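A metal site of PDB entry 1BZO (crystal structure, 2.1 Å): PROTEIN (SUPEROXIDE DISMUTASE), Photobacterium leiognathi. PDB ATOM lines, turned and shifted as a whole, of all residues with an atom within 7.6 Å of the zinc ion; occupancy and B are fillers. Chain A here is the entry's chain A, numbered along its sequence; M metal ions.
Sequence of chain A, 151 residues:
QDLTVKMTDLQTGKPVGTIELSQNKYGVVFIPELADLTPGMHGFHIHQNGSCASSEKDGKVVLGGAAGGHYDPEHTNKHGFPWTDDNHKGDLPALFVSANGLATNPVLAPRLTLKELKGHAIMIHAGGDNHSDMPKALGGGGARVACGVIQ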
ATOM      1  N   PHE A  44      -6.276   7.757 -18.005  1.00  0.00           N
ATOM      2  CA  PHE A  44      -7.596   8.018 -17.486  1.00  0.00           C
ATOM      3  C   PHE A  44      -8.617   7.441 -18.482  1.00  0.00           C
ATOM      4  O   PHE A  44      -8.568   7.851 -19.629  1.00  0.00           O
ATOM      5  CB  PHE A  44      -7.708   9.544 -17.566  1.00  0.00           C
ATOM      6  CG  PHE A  44      -8.927  10.229 -16.948  1.00  0.00           C
ATOM      7  CD1 PHE A  44      -9.511   9.768 -15.769  1.00  0.00           C
ATOM      8  CD2 PHE A  44      -9.392  11.431 -17.510  1.00  0.00           C
ATOM      9  CE1 PHE A  44     -10.602  10.433 -15.178  1.00  0.00           C
ATOM     10  CE2 PHE A  44     -10.399  12.161 -16.880  1.00  0.00           C
ATOM     11  CZ  PHE A  44     -10.996  11.664 -15.716  1.00  0.00           C
ATOM     12  N   HIS A  45      -9.540   6.505 -18.082  1.00  0.00           N
ATOM     13  CA  HIS A  45     -10.503   5.852 -19.022  1.00  0.00           C
ATOM     14  C   HIS A  45     -11.784   5.453 -18.334  1.00  0.00           C
ATOM     15  O   HIS A  45     -11.830   5.314 -17.079  1.00  0.00           O
ATOM     16  CB  HIS A  45      -9.906   4.532 -19.553  1.00  0.00           C
ATOM     17  CG  HIS A  45      -8.447   4.535 -19.755  1.00  0.00           C
ATOM     18  ND1 HIS A  45      -7.593   3.755 -19.001  1.00  0.00           N
ATOM     19  CD2 HIS A  45      -7.670   5.281 -20.603  1.00  0.00           C
ATOM     20  CE1 HIS A  45      -6.352   3.981 -19.424  1.00  0.00           C
ATOM     21  NE2 HIS A  45      -6.363   4.910 -20.405  1.00  0.00           N
ATOM     22  N   ILE A  46     -12.796   5.246 -19.167  1.00  0.00           N
ATOM     23  CA  ILE A  46     -14.099   4.739 -18.733  1.00  0.00           C
ATOM     24  C   ILE A  46     -13.938   3.243 -18.900  1.00  0.00           C
ATOM     25  O   ILE A  46     -13.410   2.822 -19.953  1.00  0.00           O
ATOM     26  CB  ILE A  46     -15.297   5.170 -19.606  1.00  0.00           C
ATOM     27  CG1 ILE A  46     -15.322   6.697 -19.805  1.00  0.00           C
ATOM     28  CG2 ILE A  46     -16.647   4.668 -19.007  1.00  0.00           C
ATOM     29  CD1 ILE A  46     -15.641   7.542 -18.563  1.00  0.00           C
ATOM     30  N   HIS A  47     -14.226   2.501 -17.825  1.00  0.00           N
ATOM     31  CA  HIS A  47     -14.164   1.032 -17.811  1.00  0.00           C
ATOM     32  C   HIS A  47     -15.584   0.490 -17.924  1.00  0.00           C
ATOM     33  O   HIS A  47     -16.590   1.231 -17.685  1.00  0.00           O
ATOM     34  CB  HIS A  47     -13.370   0.410 -16.612  1.00  0.00           C
ATOM     35  CG  HIS A  47     -11.903   0.475 -16.822  1.00  0.00           C
ATOM     36  ND1 HIS A  47     -11.113  -0.659 -16.819  1.00  0.00           N
ATOM     37  CD2 HIS A  47     -11.097   1.570 -16.987  1.00  0.00           C
ATOM     38  CE1 HIS A  47      -9.850  -0.259 -17.019  1.00  0.00           C
ATOM     39  NE2 HIS A  47      -9.822   1.071 -17.156  1.00  0.00           N
ATOM     40  N   GLY A  69     -12.499  -4.243 -18.401  1.00  0.00           N
ATOM     41  CA  GLY A  69     -11.587  -3.573 -19.349  1.00  0.00           C
ATOM     42  C   GLY A  69     -12.085  -2.183 -19.699  1.00  0.00           C
ATOM     43  O   GLY A  69     -13.066  -1.754 -19.118  1.00  0.00           O
ATOM     44  N   HIS A  70     -11.502  -1.526 -20.706  1.00  0.00           N
ATOM     45  CA  HIS A  70     -11.959  -0.162 -21.167  1.00  0.00           C
ATOM     46  C   HIS A  70     -13.387  -0.182 -21.783  1.00  0.00           C
ATOM     47  O   HIS A  70     -13.822  -1.122 -22.451  1.00  0.00           O
ATOM     48  CB  HIS A  70     -10.941   0.392 -22.226  1.00  0.00           C
ATOM     49  CG  HIS A  70      -9.569   0.618 -21.653  1.00  0.00           C
ATOM     50  ND1 HIS A  70      -8.544   1.231 -22.393  1.00  0.00           N
ATOM     51  CD2 HIS A  70      -9.103   0.397 -20.356  1.00  0.00           C
ATOM     52  CE1 HIS A  70      -7.488   1.375 -21.567  1.00  0.00           C
ATOM     53  NE2 HIS A  70      -7.781   0.860 -20.329  1.00  0.00           N
ATOM     54  N   TYR A  71     -14.160   0.861 -21.634  1.00  0.00           N
ATOM     55  CA  TYR A  71     -15.490   0.884 -22.258  1.00  0.00           C
ATOM     56  C   TYR A  71     -15.265   0.741 -23.774  1.00  0.00           C
ATOM     57  O   TYR A  71     -14.445   1.424 -24.378  1.00  0.00           O
ATOM     58  CB  TYR A  71     -16.240   2.204 -21.855  1.00  0.00           C
ATOM     59  CG  TYR A  71     -17.619   2.469 -22.481  1.00  0.00           C
ATOM     60  CD1 TYR A  71     -18.637   1.509 -22.499  1.00  0.00           C
ATOM     61  CD2 TYR A  71     -17.890   3.711 -23.057  1.00  0.00           C
ATOM     62  CE1 TYR A  71     -19.912   1.784 -23.015  1.00  0.00           C
ATOM     63  CE2 TYR A  71     -19.121   4.010 -23.642  1.00  0.00           C
ATOM     64  CZ  TYR A  71     -20.143   3.034 -23.592  1.00  0.00           C
ATOM     65  OH  TYR A  71     -21.380   3.330 -24.107  1.00  0.00           O
ATOM     66  N   ASP A  72     -15.953  -0.193 -24.420  1.00  0.00           N
ATOM     67  CA  ASP A  72     -15.768  -0.494 -25.858  1.00  0.00           C
ATOM     68  C   ASP A  72     -17.078  -0.960 -26.522  1.00  0.00           C
ATOM     69  O   ASP A  72     -17.204  -2.125 -26.952  1.00  0.00           O
ATOM     70  CB  ASP A  72     -14.730  -1.614 -26.027  1.00  0.00           C
ATOM     71  CG  ASP A  72     -14.284  -1.817 -27.449  1.00  0.00           C
ATOM     72  OD1 ASP A  72     -14.517  -1.016 -28.321  1.00  0.00           O
ATOM     73  OD2 ASP A  72     -13.471  -2.834 -27.583  1.00  0.00           O
ATOM     74  N   THR A  76     -14.065  -2.773 -30.457  1.00  0.00           N
ATOM     75  CA  THR A  76     -12.884  -2.599 -31.307  1.00  0.00           C
ATOM     76  C   THR A  76     -11.728  -3.494 -30.884  1.00  0.00           C
ATOM     77  O   THR A  76     -10.860  -3.886 -31.689  1.00  0.00           O
ATOM     78  CB  THR A  76     -12.401  -1.140 -31.271  1.00  0.00           C
ATOM     79  OG1 THR A  76     -12.064  -0.797 -29.928  1.00  0.00           O
ATOM     80  CG2 THR A  76     -13.620  -0.352 -31.760  1.00  0.00           C
ATOM     81  N   LYS A  78      -9.192  -2.491 -29.424  1.00  0.00           N
ATOM     82  CA  LYS A  78      -7.971  -1.749 -29.602  1.00  0.00           C
ATOM     83  C   LYS A  78      -7.999  -0.526 -28.661  1.00  0.00           C
ATOM     84  O   LYS A  78      -9.074   0.009 -28.262  1.00  0.00           O
ATOM     85  CB  LYS A  78      -7.896  -1.264 -31.015  1.00  0.00           C
ATOM     86  CG  LYS A  78      -7.619  -2.347 -32.067  1.00  0.00           C
ATOM     87  CD  LYS A  78      -7.597  -1.759 -33.494  1.00  0.00           C
ATOM     88  CE  LYS A  78      -7.424  -2.747 -34.655  1.00  0.00           C
ATOM     89  NZ  LYS A  78      -8.080  -4.055 -34.467  1.00  0.00           N
ATOM     90  N   HIS A  79      -6.786  -0.081 -28.270  1.00  0.00           N
ATOM     91  CA  HIS A  79      -6.627   1.105 -27.428  1.00  0.00           C
ATOM     92  C   HIS A  79      -6.119   2.295 -28.248  1.00  0.00           C
ATOM     93  O   HIS A  79      -5.178   2.194 -29.032  1.00  0.00           O
ATOM     94  CB  HIS A  79      -5.733   0.848 -26.221  1.00  0.00           C
ATOM     95  CG  HIS A  79      -5.638   2.084 -25.365  1.00  0.00           C
ATOM     96  ND1 HIS A  79      -6.692   2.505 -24.617  1.00  0.00           N
ATOM     97  CD2 HIS A  79      -4.578   2.936 -25.133  1.00  0.00           C
ATOM     98  CE1 HIS A  79      -6.297   3.563 -23.917  1.00  0.00           C
ATOM     99  NE2 HIS A  79      -5.001   3.849 -24.203  1.00  0.00           N
ATOM    100  N   GLY A  80      -6.727   3.465 -28.094  1.00  0.00           N
ATOM    101  CA  GLY A  80      -6.236   4.570 -28.943  1.00  0.00           C
ATOM    102  C   GLY A  80      -6.438   5.963 -28.369  1.00  0.00           C
ATOM    103  O   GLY A  80      -6.331   6.192 -27.140  1.00  0.00           O
ATOM    104  N   PHE A  81      -6.719   6.885 -29.292  1.00  0.00           N
ATOM    105  CA  PHE A  81      -6.913   8.344 -29.024  1.00  0.00           C
ATOM    106  C   PHE A  81      -8.363   8.704 -28.786  1.00  0.00           C
ATOM    107  O   PHE A  81      -9.295   7.994 -29.201  1.00  0.00           O
ATOM    108  CB  PHE A  81      -6.401   9.277 -30.163  1.00  0.00           C
ATOM    109  CG  PHE A  81      -4.904   9.257 -30.363  1.00  0.00           C
ATOM    110  CD1 PHE A  81      -4.070  10.110 -29.627  1.00  0.00           C
ATOM    111  CD2 PHE A  81      -4.338   8.386 -31.292  1.00  0.00           C
ATOM    112  CE1 PHE A  81      -2.686  10.022 -29.755  1.00  0.00           C
ATOM    113  CE2 PHE A  81      -2.953   8.324 -31.467  1.00  0.00           C
ATOM    114  CZ  PHE A  81      -2.131   9.138 -30.670  1.00  0.00           C
ATOM    115  N   ASN A  87     -11.230   2.390 -31.693  1.00  0.00           N
ATOM    116  CA  ASN A  87     -10.558   1.909 -30.471  1.00  0.00           C
ATOM    117  C   ASN A  87     -11.518   2.147 -29.370  1.00  0.00           C
ATOM    118  O   ASN A  87     -12.530   2.702 -29.671  1.00  0.00           O
ATOM    119  CB  ASN A  87      -9.231   2.681 -30.154  1.00  0.00           C
ATOM    120  CG  ASN A  87      -9.259   4.213 -30.286  1.00  0.00           C
ATOM    121  OD1 ASN A  87      -8.983   4.772 -31.347  1.00  0.00           O
ATOM    122  ND2 ASN A  87      -9.586   4.904 -29.208  1.00  0.00           N
ATOM    123  N   HIS A  88     -11.217   1.785 -28.142  1.00  0.00           N
ATOM    124  CA  HIS A  88     -12.219   1.951 -27.114  1.00  0.00           C
ATOM    125  C   HIS A  88     -12.894   3.299 -27.052  1.00  0.00           C
ATOM    126  O   HIS A  88     -12.261   4.356 -27.040  1.00  0.00           O
ATOM    127  CB  HIS A  88     -11.638   1.731 -25.722  1.00  0.00           C
ATOM    128  CG  HIS A  88     -10.765   0.536 -25.741  1.00  0.00           C
ATOM    129  ND1 HIS A  88      -9.480   0.540 -25.203  1.00  0.00           N
ATOM    130  CD2 HIS A  88     -10.981  -0.686 -26.250  1.00  0.00           C
ATOM    131  CE1 HIS A  88      -8.980  -0.659 -25.353  1.00  0.00           C
ATOM    132  NE2 HIS A  88      -9.868  -1.415 -26.010  1.00  0.00           N
ATOM    133  N   LYS A  89     -14.215   3.225 -26.906  1.00  0.00           N
ATOM    134  CA  LYS A  89     -15.015   4.381 -26.725  1.00  0.00           C
ATOM    135  C   LYS A  89     -14.610   5.018 -25.383  1.00  0.00           C
ATOM    136  O   LYS A  89     -14.672   6.221 -25.211  1.00  0.00           O
ATOM    137  CB  LYS A  89     -16.544   4.152 -26.940  1.00  0.00           C
ATOM    138  CG  LYS A  89     -17.172   5.383 -27.540  1.00  0.00           C
ATOM    139  CD  LYS A  89     -18.422   5.206 -28.416  1.00  0.00           C
ATOM    140  N   GLY A  90     -14.126   4.259 -24.391  1.00  0.00           N
ATOM    141  CA  GLY A  90     -13.818   5.030 -23.135  1.00  0.00           C
ATOM    142  C   GLY A  90     -12.380   5.555 -22.966  1.00  0.00           C
ATOM    143  O   GLY A  90     -11.931   5.850 -21.866  1.00  0.00           O
ATOM    144  N   ASP A  91     -11.664   5.707 -24.041  1.00  0.00           N
ATOM    145  CA  ASP A  91     -10.314   6.267 -24.000  1.00  0.00           C
ATOM    146  C   ASP A  91     -10.399   7.814 -23.924  1.00  0.00           C
ATOM    147  O   ASP A  91     -10.788   8.522 -24.875  1.00  0.00           O
ATOM    148  CB  ASP A  91      -9.611   5.895 -25.340  1.00  0.00           C
ATOM    149  CG  ASP A  91      -9.302   4.444 -25.326  1.00  0.00           C
ATOM    150  OD1 ASP A  91      -9.360   3.863 -24.245  1.00  0.00           O
ATOM    151  OD2 ASP A  91      -8.953   3.908 -26.508  1.00  0.00           O
ATOM    152  N   LEU A  92      -9.935   8.341 -22.825  1.00  0.00           N
ATOM    153  CA  LEU A  92      -9.915   9.790 -22.594  1.00  0.00           C
ATOM    154  C   LEU A  92      -8.500  10.370 -22.616  1.00  0.00           C
ATOM    155  O   LEU A  92      -7.481   9.707 -22.543  1.00  0.00           O
ATOM    156  CB  LEU A  92     -10.504  10.121 -21.203  1.00  0.00           C
ATOM    157  CG  LEU A  92     -11.761   9.308 -20.842  1.00  0.00           C
ATOM    158  CD1 LEU A  92     -12.023   9.388 -19.344  1.00  0.00           C
ATOM    159  CD2 LEU A  92     -12.945   9.875 -21.591  1.00  0.00           C
ATOM    160  N   ASP A 129      -0.383   7.474 -20.485  1.00  0.00           N
ATOM    161  CA  ASP A 129      -1.247   6.960 -21.527  1.00  0.00           C
ATOM    162  C   ASP A 129      -0.642   7.324 -22.871  1.00  0.00           C
ATOM    163  O   ASP A 129      -0.771   8.487 -23.243  1.00  0.00           O
ATOM    164  CB  ASP A 129      -2.726   7.439 -21.440  1.00  0.00           C
ATOM    165  CG  ASP A 129      -3.592   6.662 -22.433  1.00  0.00           C
ATOM    166  OD1 ASP A 129      -3.131   6.088 -23.392  1.00  0.00           O
ATOM    167  OD2 ASP A 129      -4.874   6.563 -22.149  1.00  0.00           O
ATOM    168  N   HIS A 131      -1.713   6.177 -25.772  1.00  0.00           N
ATOM    169  CA  HIS A 131      -2.752   6.012 -26.775  1.00  0.00           C
ATOM    170  C   HIS A 131      -2.399   5.020 -27.902  1.00  0.00           C
ATOM    171  O   HIS A 131      -2.684   5.235 -29.087  1.00  0.00           O
ATOM    172  CB  HIS A 131      -3.209   7.357 -27.283  1.00  0.00           C
ATOM    173  CG  HIS A 131      -3.828   8.259 -26.213  1.00  0.00           C
ATOM    174  ND1 HIS A 131      -3.198   9.446 -25.747  1.00  0.00           N
ATOM    175  CD2 HIS A 131      -5.028   8.156 -25.620  1.00  0.00           C
ATOM    176  CE1 HIS A 131      -4.009  10.034 -24.884  1.00  0.00           C
ATOM    177  NE2 HIS A 131      -5.103   9.253 -24.779  1.00  0.00           N
ATOM    178  N   SER A 132      -1.855   3.878 -27.434  1.00  0.00           N
ATOM    179  CA  SER A 132      -1.426   2.739 -28.247  1.00  0.00           C
ATOM    180  C   SER A 132      -1.352   1.512 -27.358  1.00  0.00           C
ATOM    181  O   SER A 132      -1.277   1.611 -26.138  1.00  0.00           O
ATOM    182  CB  SER A 132      -0.019   3.014 -28.742  1.00  0.00           C
ATOM    183  OG  SER A 132       0.415   2.047 -29.685  1.00  0.00           O
ATOM    184  N   ASP A 133      -1.327   0.362 -27.983  1.00  0.00           N
ATOM    185  CA  ASP A 133      -1.101  -0.886 -27.323  1.00  0.00           C
ATOM    186  C   ASP A 133       0.418  -1.187 -27.441  1.00  0.00           C
ATOM    187  O   ASP A 133       0.975  -2.168 -26.956  1.00  0.00           O
ATOM    188  CB  ASP A 133      -1.971  -2.021 -27.892  1.00  0.00           C
ATOM    189  CG  ASP A 133      -3.366  -2.018 -27.315  1.00  0.00           C
ATOM    190  OD1 ASP A 133      -3.608  -2.339 -26.170  1.00  0.00           O
ATOM    191  OD2 ASP A 133      -4.300  -1.708 -28.177  1.00  0.00           O
ATOM    192  N   LEU A 138      -2.437  -1.256 -23.451  1.00  0.00           N
ATOM    193  CA  LEU A 138      -3.326  -0.248 -22.931  1.00  0.00           C
ATOM    194  C   LEU A 138      -2.680   1.101 -22.639  1.00  0.00           C
ATOM    195  O   LEU A 138      -3.059   1.803 -21.716  1.00  0.00           O
ATOM    196  CB  LEU A 138      -4.114  -0.821 -21.726  1.00  0.00           C
ATOM    197  CG  LEU A 138      -5.076  -1.951 -22.139  1.00  0.00           C
ATOM    198  CD1 LEU A 138      -5.271  -2.921 -20.989  1.00  0.00           C
ATOM    199  CD2 LEU A 138      -6.473  -1.350 -22.321  1.00  0.00           C
ATOM    200  N   GLY A 139      -1.732   1.486 -23.475  1.00  0.00           N
ATOM    201  CA  GLY A 139      -1.041   2.782 -23.330  1.00  0.00           C
ATOM    202  C   GLY A 139      -0.005   2.909 -22.199  1.00  0.00           C
ATOM    203  O   GLY A 139       0.491   4.002 -21.884  1.00  0.00           O
HETATM  204 ZN    ZN M   1      -8.490   1.959 -24.200  1.00  0.00          ZN
HETATM  205 CU    CU M   2      -8.266   2.330 -17.563  1.00  0.00          CU
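The zinc ion is bound by a ring nitrogen (ND1) of His 79 (1.9 Å), a ring nitrogen (ND1) of His 70 (1.9 Å), a ring nitrogen (ND1) of His 88 (2.0 Å) and the side-chain carboxylate of Asp 91 (2.1 Å).
Of the 25 residues printed, 4 come within 4 Å of the zinc ion.
NE2 of His 79 is in hydrogen-bond range of OD1 of Asp 129, at 3.0 Å. The backbone NH (N) of His 79 is in hydrogen-bond range of the side-chain carboxylate (OD2) of Asp 133. A ring nitrogen (NE2) of His 70 sits close to a ring nitrogen (ND1) of His 45 (3.2 Å). A ring nitrogen (NE2) of His 88 lies within hydrogen-bond range of the backbone carbonyl oxygen (O) of Lys 78 (2.8 Å). The backbone NH (N) of His 88 sits at hydrogen-bond distance from the side-chain hydroxyl (OG1) of Thr 76. The backbone NH (N) of Gly 80 lies within hydrogen-bond range of the side-chain carboxylate (OD2) of Asp 91 (2.8 Å). The side-chain amide nitrogen (ND2) of Asn 87 is in hydrogen-bond range of the side-chain carboxylate (OD2) of Asp 91.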
